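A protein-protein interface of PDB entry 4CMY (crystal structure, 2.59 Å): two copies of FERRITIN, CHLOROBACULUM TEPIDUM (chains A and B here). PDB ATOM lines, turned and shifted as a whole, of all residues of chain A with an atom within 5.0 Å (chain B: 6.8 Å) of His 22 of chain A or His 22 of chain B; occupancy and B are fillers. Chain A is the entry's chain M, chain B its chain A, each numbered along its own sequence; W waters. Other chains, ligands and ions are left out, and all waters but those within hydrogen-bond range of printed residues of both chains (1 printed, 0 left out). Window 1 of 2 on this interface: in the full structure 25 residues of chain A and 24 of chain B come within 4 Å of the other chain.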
ATOM      1  N   ALA A  18     -33.988 -25.754  -5.303  1.00  0.00           N
ATOM      2  CA  ALA A  18     -32.704 -25.105  -5.051  1.00  0.00           C
ATOM      3  C   ALA A  18     -31.804 -25.989  -4.183  1.00  0.00           C
ATOM      4  O   ALA A  18     -30.612 -26.107  -4.454  1.00  0.00           O
ATOM      5  CB  ALA A  18     -32.911 -23.774  -4.366  1.00  0.00           C
ATOM      6  N   ALA A  19     -32.375 -26.581  -3.144  1.00  0.00           N
ATOM      7  CA  ALA A  19     -31.613 -27.454  -2.271  1.00  0.00           C
ATOM      8  C   ALA A  19     -31.123 -28.692  -3.019  1.00  0.00           C
ATOM      9  O   ALA A  19     -30.050 -29.218  -2.711  1.00  0.00           O
ATOM     10  CB  ALA A  19     -32.427 -27.878  -1.078  1.00  0.00           C
ATOM     11  N   SER A  20     -31.898 -29.153  -4.001  1.00  0.00           N
ATOM     12  CA  SER A  20     -31.489 -30.313  -4.793  1.00  0.00           C
ATOM     13  C   SER A  20     -30.277 -29.986  -5.632  1.00  0.00           C
ATOM     14  O   SER A  20     -29.369 -30.796  -5.760  1.00  0.00           O
ATOM     15  CB  SER A  20     -32.614 -30.792  -5.693  1.00  0.00           C
ATOM     16  OG  SER A  20     -33.773 -31.013  -4.920  1.00  0.00           O
ATOM     17  N   ALA A  21     -30.278 -28.816  -6.233  1.00  0.00           N
ATOM     18  CA  ALA A  21     -29.142 -28.419  -7.035  1.00  0.00           C
ATOM     19  C   ALA A  21     -27.860 -28.425  -6.195  1.00  0.00           C
ATOM     20  O   ALA A  21     -26.840 -28.967  -6.612  1.00  0.00           O
ATOM     21  CB  ALA A  21     -29.366 -27.043  -7.624  1.00  0.00           C
ATOM     22  N   HIS A  22     -27.941 -27.830  -5.015  1.00  0.00           N
ATOM     23  CA  HIS A  22     -26.795 -27.733  -4.134  1.00  0.00           C
ATOM     24  C   HIS A  22     -26.407 -29.104  -3.651  1.00  0.00           C
ATOM     25  O   HIS A  22     -25.215 -29.408  -3.548  1.00  0.00           O
ATOM     26  CB  HIS A  22     -27.127 -26.845  -2.923  1.00  0.00           C
ATOM     27  CG  HIS A  22     -27.026 -25.372  -3.171  1.00  0.00           C
ATOM     28  ND1 HIS A  22     -27.239 -24.817  -4.414  1.00  0.00           N
ATOM     29  CD2 HIS A  22     -26.861 -24.331  -2.327  1.00  0.00           C
ATOM     30  CE1 HIS A  22     -27.196 -23.503  -4.334  1.00  0.00           C
ATOM     31  NE2 HIS A  22     -26.973 -23.183  -3.079  1.00  0.00           N
ATOM     32  N   LEU A  23     -27.392 -29.953  -3.349  1.00  0.00           N
ATOM     33  CA  LEU A  23     -27.076 -31.329  -2.931  1.00  0.00           C
ATOM     34  C   LEU A  23     -26.286 -32.069  -4.020  1.00  0.00           C
ATOM     35  O   LEU A  23     -25.291 -32.709  -3.732  1.00  0.00           O
ATOM     36  CB  LEU A  23     -28.342 -32.097  -2.606  1.00  0.00           C
ATOM     37  CG  LEU A  23     -28.202 -33.563  -2.130  1.00  0.00           C
ATOM     38  CD1 LEU A  23     -27.391 -33.649  -0.854  1.00  0.00           C
ATOM     39  CD2 LEU A  23     -29.569 -34.231  -1.930  1.00  0.00           C
ATOM     40  N   TYR A  24     -26.702 -31.924  -5.268  1.00  0.00           N
ATOM     41  CA  TYR A  24     -26.070 -32.660  -6.321  1.00  0.00           C
ATOM     42  C   TYR A  24     -24.699 -32.111  -6.636  1.00  0.00           C
ATOM     43  O   TYR A  24     -23.796 -32.843  -7.019  1.00  0.00           O
ATOM     44  CB  TYR A  24     -26.990 -32.745  -7.546  1.00  0.00           C
ATOM     45  CG  TYR A  24     -28.271 -33.547  -7.335  1.00  0.00           C
ATOM     46  CD1 TYR A  24     -28.355 -34.564  -6.380  1.00  0.00           C
ATOM     47  CD2 TYR A  24     -29.395 -33.312  -8.124  1.00  0.00           C
ATOM     48  CE1 TYR A  24     -29.526 -35.267  -6.178  1.00  0.00           C
ATOM     49  CE2 TYR A  24     -30.566 -34.015  -7.931  1.00  0.00           C
ATOM     50  CZ  TYR A  24     -30.627 -34.996  -6.956  1.00  0.00           C
ATOM     51  OH  TYR A  24     -31.773 -35.740  -6.796  1.00  0.00           O
ATOM     52  N   LEU A  25     -24.530 -30.812  -6.507  1.00  0.00           N
ATOM     53  CA  LEU A  25     -23.189 -30.231  -6.622  1.00  0.00           C
ATOM     54  C   LEU A  25     -22.287 -30.824  -5.573  1.00  0.00           C
ATOM     55  O   LEU A  25     -21.165 -31.227  -5.861  1.00  0.00           O
ATOM     56  CB  LEU A  25     -23.239 -28.721  -6.432  1.00  0.00           C
ATOM     57  CG  LEU A  25     -23.018 -27.808  -7.625  1.00  0.00           C
ATOM     58  CD1 LEU A  25     -23.157 -28.455  -8.980  1.00  0.00           C
ATOM     59  CD2 LEU A  25     -23.977 -26.628  -7.528  1.00  0.00           C
ATOM     60  N   GLN A  26     -22.774 -30.892  -4.336  1.00  0.00           N
ATOM     61  CA  GLN A  26     -21.958 -31.412  -3.241  1.00  0.00           C
ATOM     62  C   GLN A  26     -21.597 -32.878  -3.468  1.00  0.00           C
ATOM     63  O   GLN A  26     -20.477 -33.299  -3.185  1.00  0.00           O
ATOM     64  CB  GLN A  26     -22.668 -31.216  -1.913  1.00  0.00           C
ATOM     65  CG  GLN A  26     -21.786 -31.456  -0.696  1.00  0.00           C
ATOM     66  CD  GLN A  26     -20.613 -30.518  -0.634  1.00  0.00           C
ATOM     67  OE1 GLN A  26     -20.705 -29.410  -0.101  1.00  0.00           O
ATOM     68  NE2 GLN A  26     -19.488 -30.962  -1.171  1.00  0.00           N
ATOM     69  N   ILE A  70     -36.909 -17.566  -2.295  1.00  0.00           N
ATOM     70  CA  ILE A  70     -35.902 -18.600  -2.360  1.00  0.00           C
ATOM     71  C   ILE A  70     -35.736 -19.281  -1.010  1.00  0.00           C
ATOM     72  O   ILE A  70     -35.581 -20.510  -0.946  1.00  0.00           O
ATOM     73  CB  ILE A  70     -34.522 -18.033  -2.751  1.00  0.00           C
ATOM     74  CG1 ILE A  70     -34.625 -17.125  -3.986  1.00  0.00           C
ATOM     75  CG2 ILE A  70     -33.551 -19.167  -3.005  1.00  0.00           C
ATOM     76  CD1 ILE A  70     -34.937 -17.863  -5.266  1.00  0.00           C
ATOM     77  N   VAL A  73     -31.284 -22.422   2.231  1.00  0.00           N
ATOM     78  CA  VAL A  73     -30.909 -23.701   1.655  1.00  0.00           C
ATOM     79  C   VAL A  73     -29.677 -24.172   2.390  1.00  0.00           C
ATOM     80  O   VAL A  73     -28.654 -23.476   2.369  1.00  0.00           O
ATOM     81  CB  VAL A  73     -30.566 -23.514   0.179  1.00  0.00           C
ATOM     82  CG1 VAL A  73     -30.173 -24.818  -0.428  1.00  0.00           C
ATOM     83  CG2 VAL A  73     -31.744 -22.938  -0.581  1.00  0.00           C
ATOM     84  N   THR A  75     -26.866 -27.174   2.926  1.00  0.00           N
ATOM     85  CA  THR A  75     -26.338 -28.412   2.360  1.00  0.00           C
ATOM     86  C   THR A  75     -25.332 -29.010   3.300  1.00  0.00           C
ATOM     87  O   THR A  75     -24.296 -28.402   3.569  1.00  0.00           O
ATOM     88  CB  THR A  75     -25.660 -28.188   1.016  1.00  0.00           C
ATOM     89  OG1 THR A  75     -26.554 -27.469   0.165  1.00  0.00           O
ATOM     90  CG2 THR A  75     -25.288 -29.523   0.375  1.00  0.00           C
ATOM     91  N   GLU B  17     -20.481 -16.610  -3.419  1.00  0.00           N
ATOM     92  CA  GLU B  17     -20.976 -16.489  -4.793  1.00  0.00           C
ATOM     93  C   GLU B  17     -22.335 -17.159  -4.929  1.00  0.00           C
ATOM     94  O   GLU B  17     -23.249 -16.604  -5.545  1.00  0.00           O
ATOM     95  CB  GLU B  17     -19.979 -17.064  -5.810  1.00  0.00           C
ATOM     96  CG  GLU B  17     -18.596 -16.432  -5.764  1.00  0.00           C
ATOM     97  CD  GLU B  17     -18.521 -14.993  -6.282  1.00  0.00           C
ATOM     98  OE1 GLU B  17     -19.397 -14.536  -7.087  1.00  0.00           O
ATOM     99  OE2 GLU B  17     -17.479 -14.311  -5.973  1.00  0.00           O
ATOM    100  N   ALA B  18     -22.506 -18.323  -4.322  1.00  0.00           N
ATOM    101  CA  ALA B  18     -23.832 -18.977  -4.291  1.00  0.00           C
ATOM    102  C   ALA B  18     -24.899 -18.083  -3.661  1.00  0.00           C
ATOM    103  O   ALA B  18     -26.003 -17.957  -4.185  1.00  0.00           O
ATOM    104  CB  ALA B  18     -23.777 -20.269  -3.530  1.00  0.00           C
ATOM    105  N   ALA B  19     -24.547 -17.416  -2.572  1.00  0.00           N
ATOM    106  CA  ALA B  19     -25.492 -16.494  -1.930  1.00  0.00           C
ATOM    107  C   ALA B  19     -25.811 -15.295  -2.790  1.00  0.00           C
ATOM    108  O   ALA B  19     -26.914 -14.782  -2.720  1.00  0.00           O
ATOM    109  CB  ALA B  19     -24.950 -16.033  -0.586  1.00  0.00           C
ATOM    110  N   SER B  20     -24.861 -14.871  -3.595  1.00  0.00           N
ATOM    111  CA  SER B  20     -25.082 -13.747  -4.504  1.00  0.00           C
ATOM    112  C   SER B  20     -26.063 -14.092  -5.582  1.00  0.00           C
ATOM    113  O   SER B  20     -26.938 -13.321  -5.894  1.00  0.00           O
ATOM    114  CB  SER B  20     -23.772 -13.303  -5.159  1.00  0.00           C
ATOM    115  OG  SER B  20     -22.808 -13.052  -4.166  1.00  0.00           O
ATOM    116  N   ALA B  21     -25.949 -15.297  -6.116  1.00  0.00           N
ATOM    117  CA  ALA B  21     -26.909 -15.739  -7.104  1.00  0.00           C
ATOM    118  C   ALA B  21     -28.320 -15.711  -6.541  1.00  0.00           C
ATOM    119  O   ALA B  21     -29.238 -15.203  -7.182  1.00  0.00           O
ATOM    120  CB  ALA B  21     -26.572 -17.136  -7.587  1.00  0.00           C
ATOM    121  N   HIS B  22     -28.483 -16.257  -5.346  1.00  0.00           N
ATOM    122  CA  HIS B  22     -29.797 -16.336  -4.723  1.00  0.00           C
ATOM    123  C   HIS B  22     -30.299 -14.943  -4.367  1.00  0.00           C
ATOM    124  O   HIS B  22     -31.470 -14.654  -4.547  1.00  0.00           O
ATOM    125  CB  HIS B  22     -29.726 -17.175  -3.453  1.00  0.00           C
ATOM    126  CG  HIS B  22     -29.765 -18.662  -3.658  1.00  0.00           C
ATOM    127  ND1 HIS B  22     -29.306 -19.261  -4.807  1.00  0.00           N
ATOM    128  CD2 HIS B  22     -30.099 -19.673  -2.820  1.00  0.00           C
ATOM    129  CE1 HIS B  22     -29.388 -20.571  -4.690  1.00  0.00           C
ATOM    130  NE2 HIS B  22     -29.867 -20.844  -3.490  1.00  0.00           N
ATOM    131  N   LEU B  23     -29.408 -14.078  -3.893  1.00  0.00           N
ATOM    132  CA  LEU B  23     -29.774 -12.695  -3.608  1.00  0.00           C
ATOM    133  C   LEU B  23     -30.280 -11.989  -4.845  1.00  0.00           C
ATOM    134  O   LEU B  23     -31.357 -11.365  -4.828  1.00  0.00           O
ATOM    135  CB  LEU B  23     -28.585 -11.925  -3.067  1.00  0.00           C
ATOM    136  CG  LEU B  23     -28.833 -10.442  -2.713  1.00  0.00           C
ATOM    137  CD1 LEU B  23     -29.882 -10.311  -1.632  1.00  0.00           C
ATOM    138  CD2 LEU B  23     -27.559  -9.756  -2.256  1.00  0.00           C
ATOM    139  N   TYR B  24     -29.586 -12.151  -5.964  1.00  0.00           N
ATOM    140  CA  TYR B  24     -30.022 -11.483  -7.190  1.00  0.00           C
ATOM    141  C   TYR B  24     -31.314 -12.081  -7.779  1.00  0.00           C
ATOM    142  O   TYR B  24     -32.128 -11.365  -8.362  1.00  0.00           O
ATOM    143  CB  TYR B  24     -28.890 -11.446  -8.194  1.00  0.00           C
ATOM    144  CG  TYR B  24     -27.685 -10.654  -7.739  1.00  0.00           C
ATOM    145  CD1 TYR B  24     -27.792  -9.632  -6.833  1.00  0.00           C
ATOM    146  CD2 TYR B  24     -26.432 -10.905  -8.266  1.00  0.00           C
ATOM    147  CE1 TYR B  24     -26.699  -8.899  -6.449  1.00  0.00           C
ATOM    148  CE2 TYR B  24     -25.346 -10.168  -7.890  1.00  0.00           C
ATOM    149  CZ  TYR B  24     -25.486  -9.159  -6.981  1.00  0.00           C
ATOM    150  OH  TYR B  24     -24.372  -8.411  -6.598  1.00  0.00           O
ATOM    151  N   LEU B  25     -31.517 -13.379  -7.627  1.00  0.00           N
ATOM    152  CA  LEU B  25     -32.802 -13.962  -7.993  1.00  0.00           C
ATOM    153  C   LEU B  25     -33.921 -13.310  -7.188  1.00  0.00           C
ATOM    154  O   LEU B  25     -34.950 -12.948  -7.718  1.00  0.00           O
ATOM    155  CB  LEU B  25     -32.794 -15.459  -7.722  1.00  0.00           C
ATOM    156  CG  LEU B  25     -32.762 -16.436  -8.892  1.00  0.00           C
ATOM    157  CD1 LEU B  25     -32.352 -15.839 -10.230  1.00  0.00           C
ATOM    158  CD2 LEU B  25     -31.857 -17.584  -8.545  1.00  0.00           C
ATOM    159  N   GLN B  26     -33.705 -13.181  -5.882  1.00  0.00           N
ATOM    160  CA  GLN B  26     -34.726 -12.645  -5.002  1.00  0.00           C
ATOM    161  C   GLN B  26     -35.017 -11.193  -5.340  1.00  0.00           C
ATOM    162  O   GLN B  26     -36.175 -10.777  -5.323  1.00  0.00           O
ATOM    163  CB  GLN B  26     -34.312 -12.796  -3.542  1.00  0.00           C
ATOM    164  CG  GLN B  26     -35.415 -12.508  -2.547  1.00  0.00           C
ATOM    165  CD  GLN B  26     -36.592 -13.450  -2.699  1.00  0.00           C
ATOM    166  OE1 GLN B  26     -36.616 -14.545  -2.121  1.00  0.00           O
ATOM    167  NE2 GLN B  26     -37.572 -13.033  -3.479  1.00  0.00           N
ATOM    168  N   MET B  27     -33.981 -10.449  -5.677  1.00  0.00           N
ATOM    169  CA  MET B  27     -34.165  -9.075  -6.091  1.00  0.00           C
ATOM    170  C   MET B  27     -34.986  -9.023  -7.374  1.00  0.00           C
ATOM    171  O   MET B  27     -35.859  -8.178  -7.513  1.00  0.00           O
ATOM    172  CB  MET B  27     -32.807  -8.365  -6.303  1.00  0.00           C
ATOM    173  CG  MET B  27     -32.049  -8.036  -5.021  1.00  0.00           C
ATOM    174  SD  MET B  27     -30.443  -7.302  -5.356  1.00  0.00           S
ATOM    175  CE  MET B  27     -29.963  -6.826  -3.704  1.00  0.00           C
ATOM    176  N   ALA B  47     -27.757 -13.308 -11.871  1.00  0.00           N
ATOM    177  CA  ALA B  47     -27.711 -14.439 -10.974  1.00  0.00           C
ATOM    178  C   ALA B  47     -26.999 -15.590 -11.667  1.00  0.00           C
ATOM    179  O   ALA B  47     -26.271 -16.334 -11.030  1.00  0.00           O
ATOM    180  CB  ALA B  47     -29.104 -14.864 -10.557  1.00  0.00           C
ATOM    181  N   GLU B  50     -23.243 -15.057 -11.378  1.00  0.00           N
ATOM    182  CA  GLU B  50     -22.726 -15.395 -10.060  1.00  0.00           C
ATOM    183  C   GLU B  50     -22.583 -16.898  -9.911  1.00  0.00           C
ATOM    184  O   GLU B  50     -21.670 -17.381  -9.277  1.00  0.00           O
ATOM    185  CB  GLU B  50     -23.585 -14.790  -8.937  1.00  0.00           C
ATOM    186  CG  GLU B  50     -23.619 -13.269  -8.965  1.00  0.00           C
ATOM    187  CD  GLU B  50     -22.271 -12.568  -8.716  1.00  0.00           C
ATOM    188  OE1 GLU B  50     -21.305 -13.260  -8.282  1.00  0.00           O
ATOM    189  OE2 GLU B  50     -22.210 -11.285  -8.935  1.00  0.00           O
ATOM    190  N   MET B  54     -19.231 -19.033  -8.981  1.00  0.00           N
ATOM    191  CA  MET B  54     -19.231 -20.098  -7.992  1.00  0.00           C
ATOM    192  C   MET B  54     -18.591 -21.357  -8.558  1.00  0.00           C
ATOM    193  O   MET B  54     -17.707 -21.934  -7.909  1.00  0.00           O
ATOM    194  CB  MET B  54     -20.646 -20.395  -7.521  1.00  0.00           C
ATOM    195  CG  MET B  54     -20.722 -21.540  -6.539  1.00  0.00           C
ATOM    196  SD  MET B  54     -22.420 -22.065  -6.245  1.00  0.00           S
ATOM    197  CE  MET B  54     -22.670 -23.022  -7.712  1.00  0.00           C
ATOM    198  N   ILE B  70     -20.293 -26.348  -0.425  1.00  0.00           N
ATOM    199  CA  ILE B  70     -21.269 -25.320  -0.722  1.00  0.00           C
ATOM    200  C   ILE B  70     -21.702 -24.586   0.538  1.00  0.00           C
ATOM    201  O   ILE B  70     -21.874 -23.371   0.510  1.00  0.00           O
ATOM    202  CB  ILE B  70     -22.536 -25.919  -1.375  1.00  0.00           C
ATOM    203  CG1 ILE B  70     -22.184 -26.865  -2.533  1.00  0.00           C
ATOM    204  CG2 ILE B  70     -23.437 -24.802  -1.892  1.00  0.00           C
ATOM    205  CD1 ILE B  70     -21.600 -26.177  -3.755  1.00  0.00           C
ATOM    206  N   GLY B  71     -21.973 -25.337   1.609  1.00  0.00           N
ATOM    207  CA  GLY B  71     -22.426 -24.766   2.859  1.00  0.00           C
ATOM    208  C   GLY B  71     -23.860 -24.322   2.897  1.00  0.00           C
ATOM    209  O   GLY B  71     -24.675 -24.752   2.087  1.00  0.00           O
ATOM    210  N   GLU B  72     -24.172 -23.443   3.843  1.00  0.00           N
ATOM    211  CA  GLU B  72     -25.527 -22.911   4.014  1.00  0.00           C
ATOM    212  C   GLU B  72     -25.643 -21.569   3.306  1.00  0.00           C
ATOM    213  O   GLU B  72     -24.791 -20.737   3.467  1.00  0.00           O
ATOM    214  CB  GLU B  72     -25.838 -22.658   5.499  1.00  0.00           C
ATOM    215  CG  GLU B  72     -25.748 -23.890   6.394  1.00  0.00           C
ATOM    216  CD  GLU B  72     -26.141 -23.611   7.846  1.00  0.00           C
ATOM    217  OE1 GLU B  72     -26.883 -22.620   8.104  1.00  0.00           O
ATOM    218  OE2 GLU B  72     -25.716 -24.409   8.726  1.00  0.00           O
ATOM    219  N   VAL B  73     -26.731 -21.361   2.595  1.00  0.00           N
ATOM    220  CA  VAL B  73     -26.985 -20.127   1.920  1.00  0.00           C
ATOM    221  C   VAL B  73     -28.354 -19.647   2.363  1.00  0.00           C
ATOM    222  O   VAL B  73     -29.347 -20.345   2.168  1.00  0.00           O
ATOM    223  CB  VAL B  73     -27.023 -20.374   0.419  1.00  0.00           C
ATOM    224  CG1 VAL B  73     -27.280 -19.086  -0.312  1.00  0.00           C
ATOM    225  CG2 VAL B  73     -25.708 -20.967  -0.060  1.00  0.00           C
ATOM    226  N   ALA B  74     -28.433 -18.487   2.996  1.00  0.00           N
ATOM    227  CA  ALA B  74     -29.731 -18.022   3.505  1.00  0.00           C
ATOM    228  C   ALA B  74     -30.064 -16.725   2.846  1.00  0.00           C
ATOM    229  O   ALA B  74     -29.301 -15.785   2.946  1.00  0.00           O
ATOM    230  CB  ALA B  74     -29.716 -17.854   5.038  1.00  0.00           C
ATOM    231  N   THR B  75     -31.215 -16.653   2.209  1.00  0.00           N
ATOM    232  CA  THR B  75     -31.599 -15.438   1.511  1.00  0.00           C
ATOM    233  C   THR B  75     -32.776 -14.816   2.220  1.00  0.00           C
ATOM    234  O   THR B  75     -33.859 -15.414   2.261  1.00  0.00           O
ATOM    235  CB  THR B  75     -31.992 -15.711   0.047  1.00  0.00           C
ATOM    236  OG1 THR B  75     -30.952 -16.456  -0.573  1.00  0.00           O
ATOM    237  CG2 THR B  75     -32.231 -14.396  -0.717  1.00  0.00           C
HETATM  238  O   HOH W   1     -26.902 -24.893   0.540  1.00  0.00           O
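Of the 12 printed residues of chain A, 6 touch a printed residue of chain B. Printed residues of chain A that touch a printed residue of chain B: His 22, Leu 25, Gln 26, Ile 70, Val 73 and Thr 75. Of the 20 printed residues of chain B, 7 touch a printed residue of chain A. Hydrophobic or aromatic side chains of chain B that line the printed part of chain A: His 22, Met 54, Ile 70 and Val 73. Among the printed residues, no Asp or Glu carboxylate lies within 4 Å of a Lys or Arg side-chain nitrogen of the other chain.
Water W1 lies within hydrogen-bond range of OG1 of Thr 75 of chain A (2.6 Å), O of Gly 71 of chain B (2.7 Å) and O of Val 73 of chain A (2.9 Å).
The side-chain amide oxygen (OE1) of Gln 26 of chain B is in hydrogen-bond range of the backbone NH (N) of Ile 70 of chain A, at 3.0 Å. N of Ile 70 of chain B sits at hydrogen-bond distance from OE1 of Gln 26 of chain A. The backbone carbonyl oxygen (O) of Gly 71 of chain B is in hydrogen-bond range of the backbone NH (N) of Thr 75 of chain A (3.4 Å). The backbone carbonyl oxygen of Val 73 of chain B sits at hydrogen-bond distance from the backbone NH of Val 73 of chain A, at 2.8 Å.
His 22 of chain A touches His 22 of chain B. CD2 of His 22 of chain A touches CG2 of Ile 70 of chain B, at 3.5 Å. Val 73 of chain B touches His 22 of chain A. Leu 25 of chain A touches Met 54 of chain B. Ile 70 of chain A touches His 22 of chain B. Glu 72 of chain B touches Val 73 of chain A (CA to O, 3.6 Å).
His 22 of chain A touches its own counterpart, His 22 of chain B. His 22 of chain A touches Ile 70 of chain B, and with the chains exchanged Ile 70 of chain A touches His 22 of chain B. His 22 of chain A touches Val 73 of chain B, but with the chains exchanged Val 73 of chain A does not touch His 22 of chain B (4.05 Å). Gln 26 of chain A touches Ile 70 of chain B, and with the chains exchanged Ile 70 of chain A touches Gln 26 of chain B. Of the 10 pairs that touch across the chains among the printed residues, 6 have their exchanged pair printed and touching as well.
His 22 of chain A touches three residues of chain B. Tyr 24 of chain A touches none of the printed residues of chain B. Of the printed residues of chain B, Leu 25 of chain A touches Met 54 (3.8 Å). Of the printed residues of chain B, Val 73 of chain A touches Glu 72 and Val 73. Of chain A, only His 22 (3.7 Å) and Ile 70 (3.5 Å) come within 4 Å of His 22 of chain B. Glu 50 of chain B touches none of the printed residues of chain A. Of the printed residues of chain A, Ile 70 of chain B touches His 22 (3.5 Å) and Gln 26 (3.1 Å). Of the printed residues of chain A, Gly 71 of chain B touches Thr 75. Of the printed residues of chain A, Glu 72 of chain B touches Val 73 (3.6 Å). The nearest printed residue of chain A that does not touch Gly 71 of chain B is Val 73 of chain A (4.2 Å).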
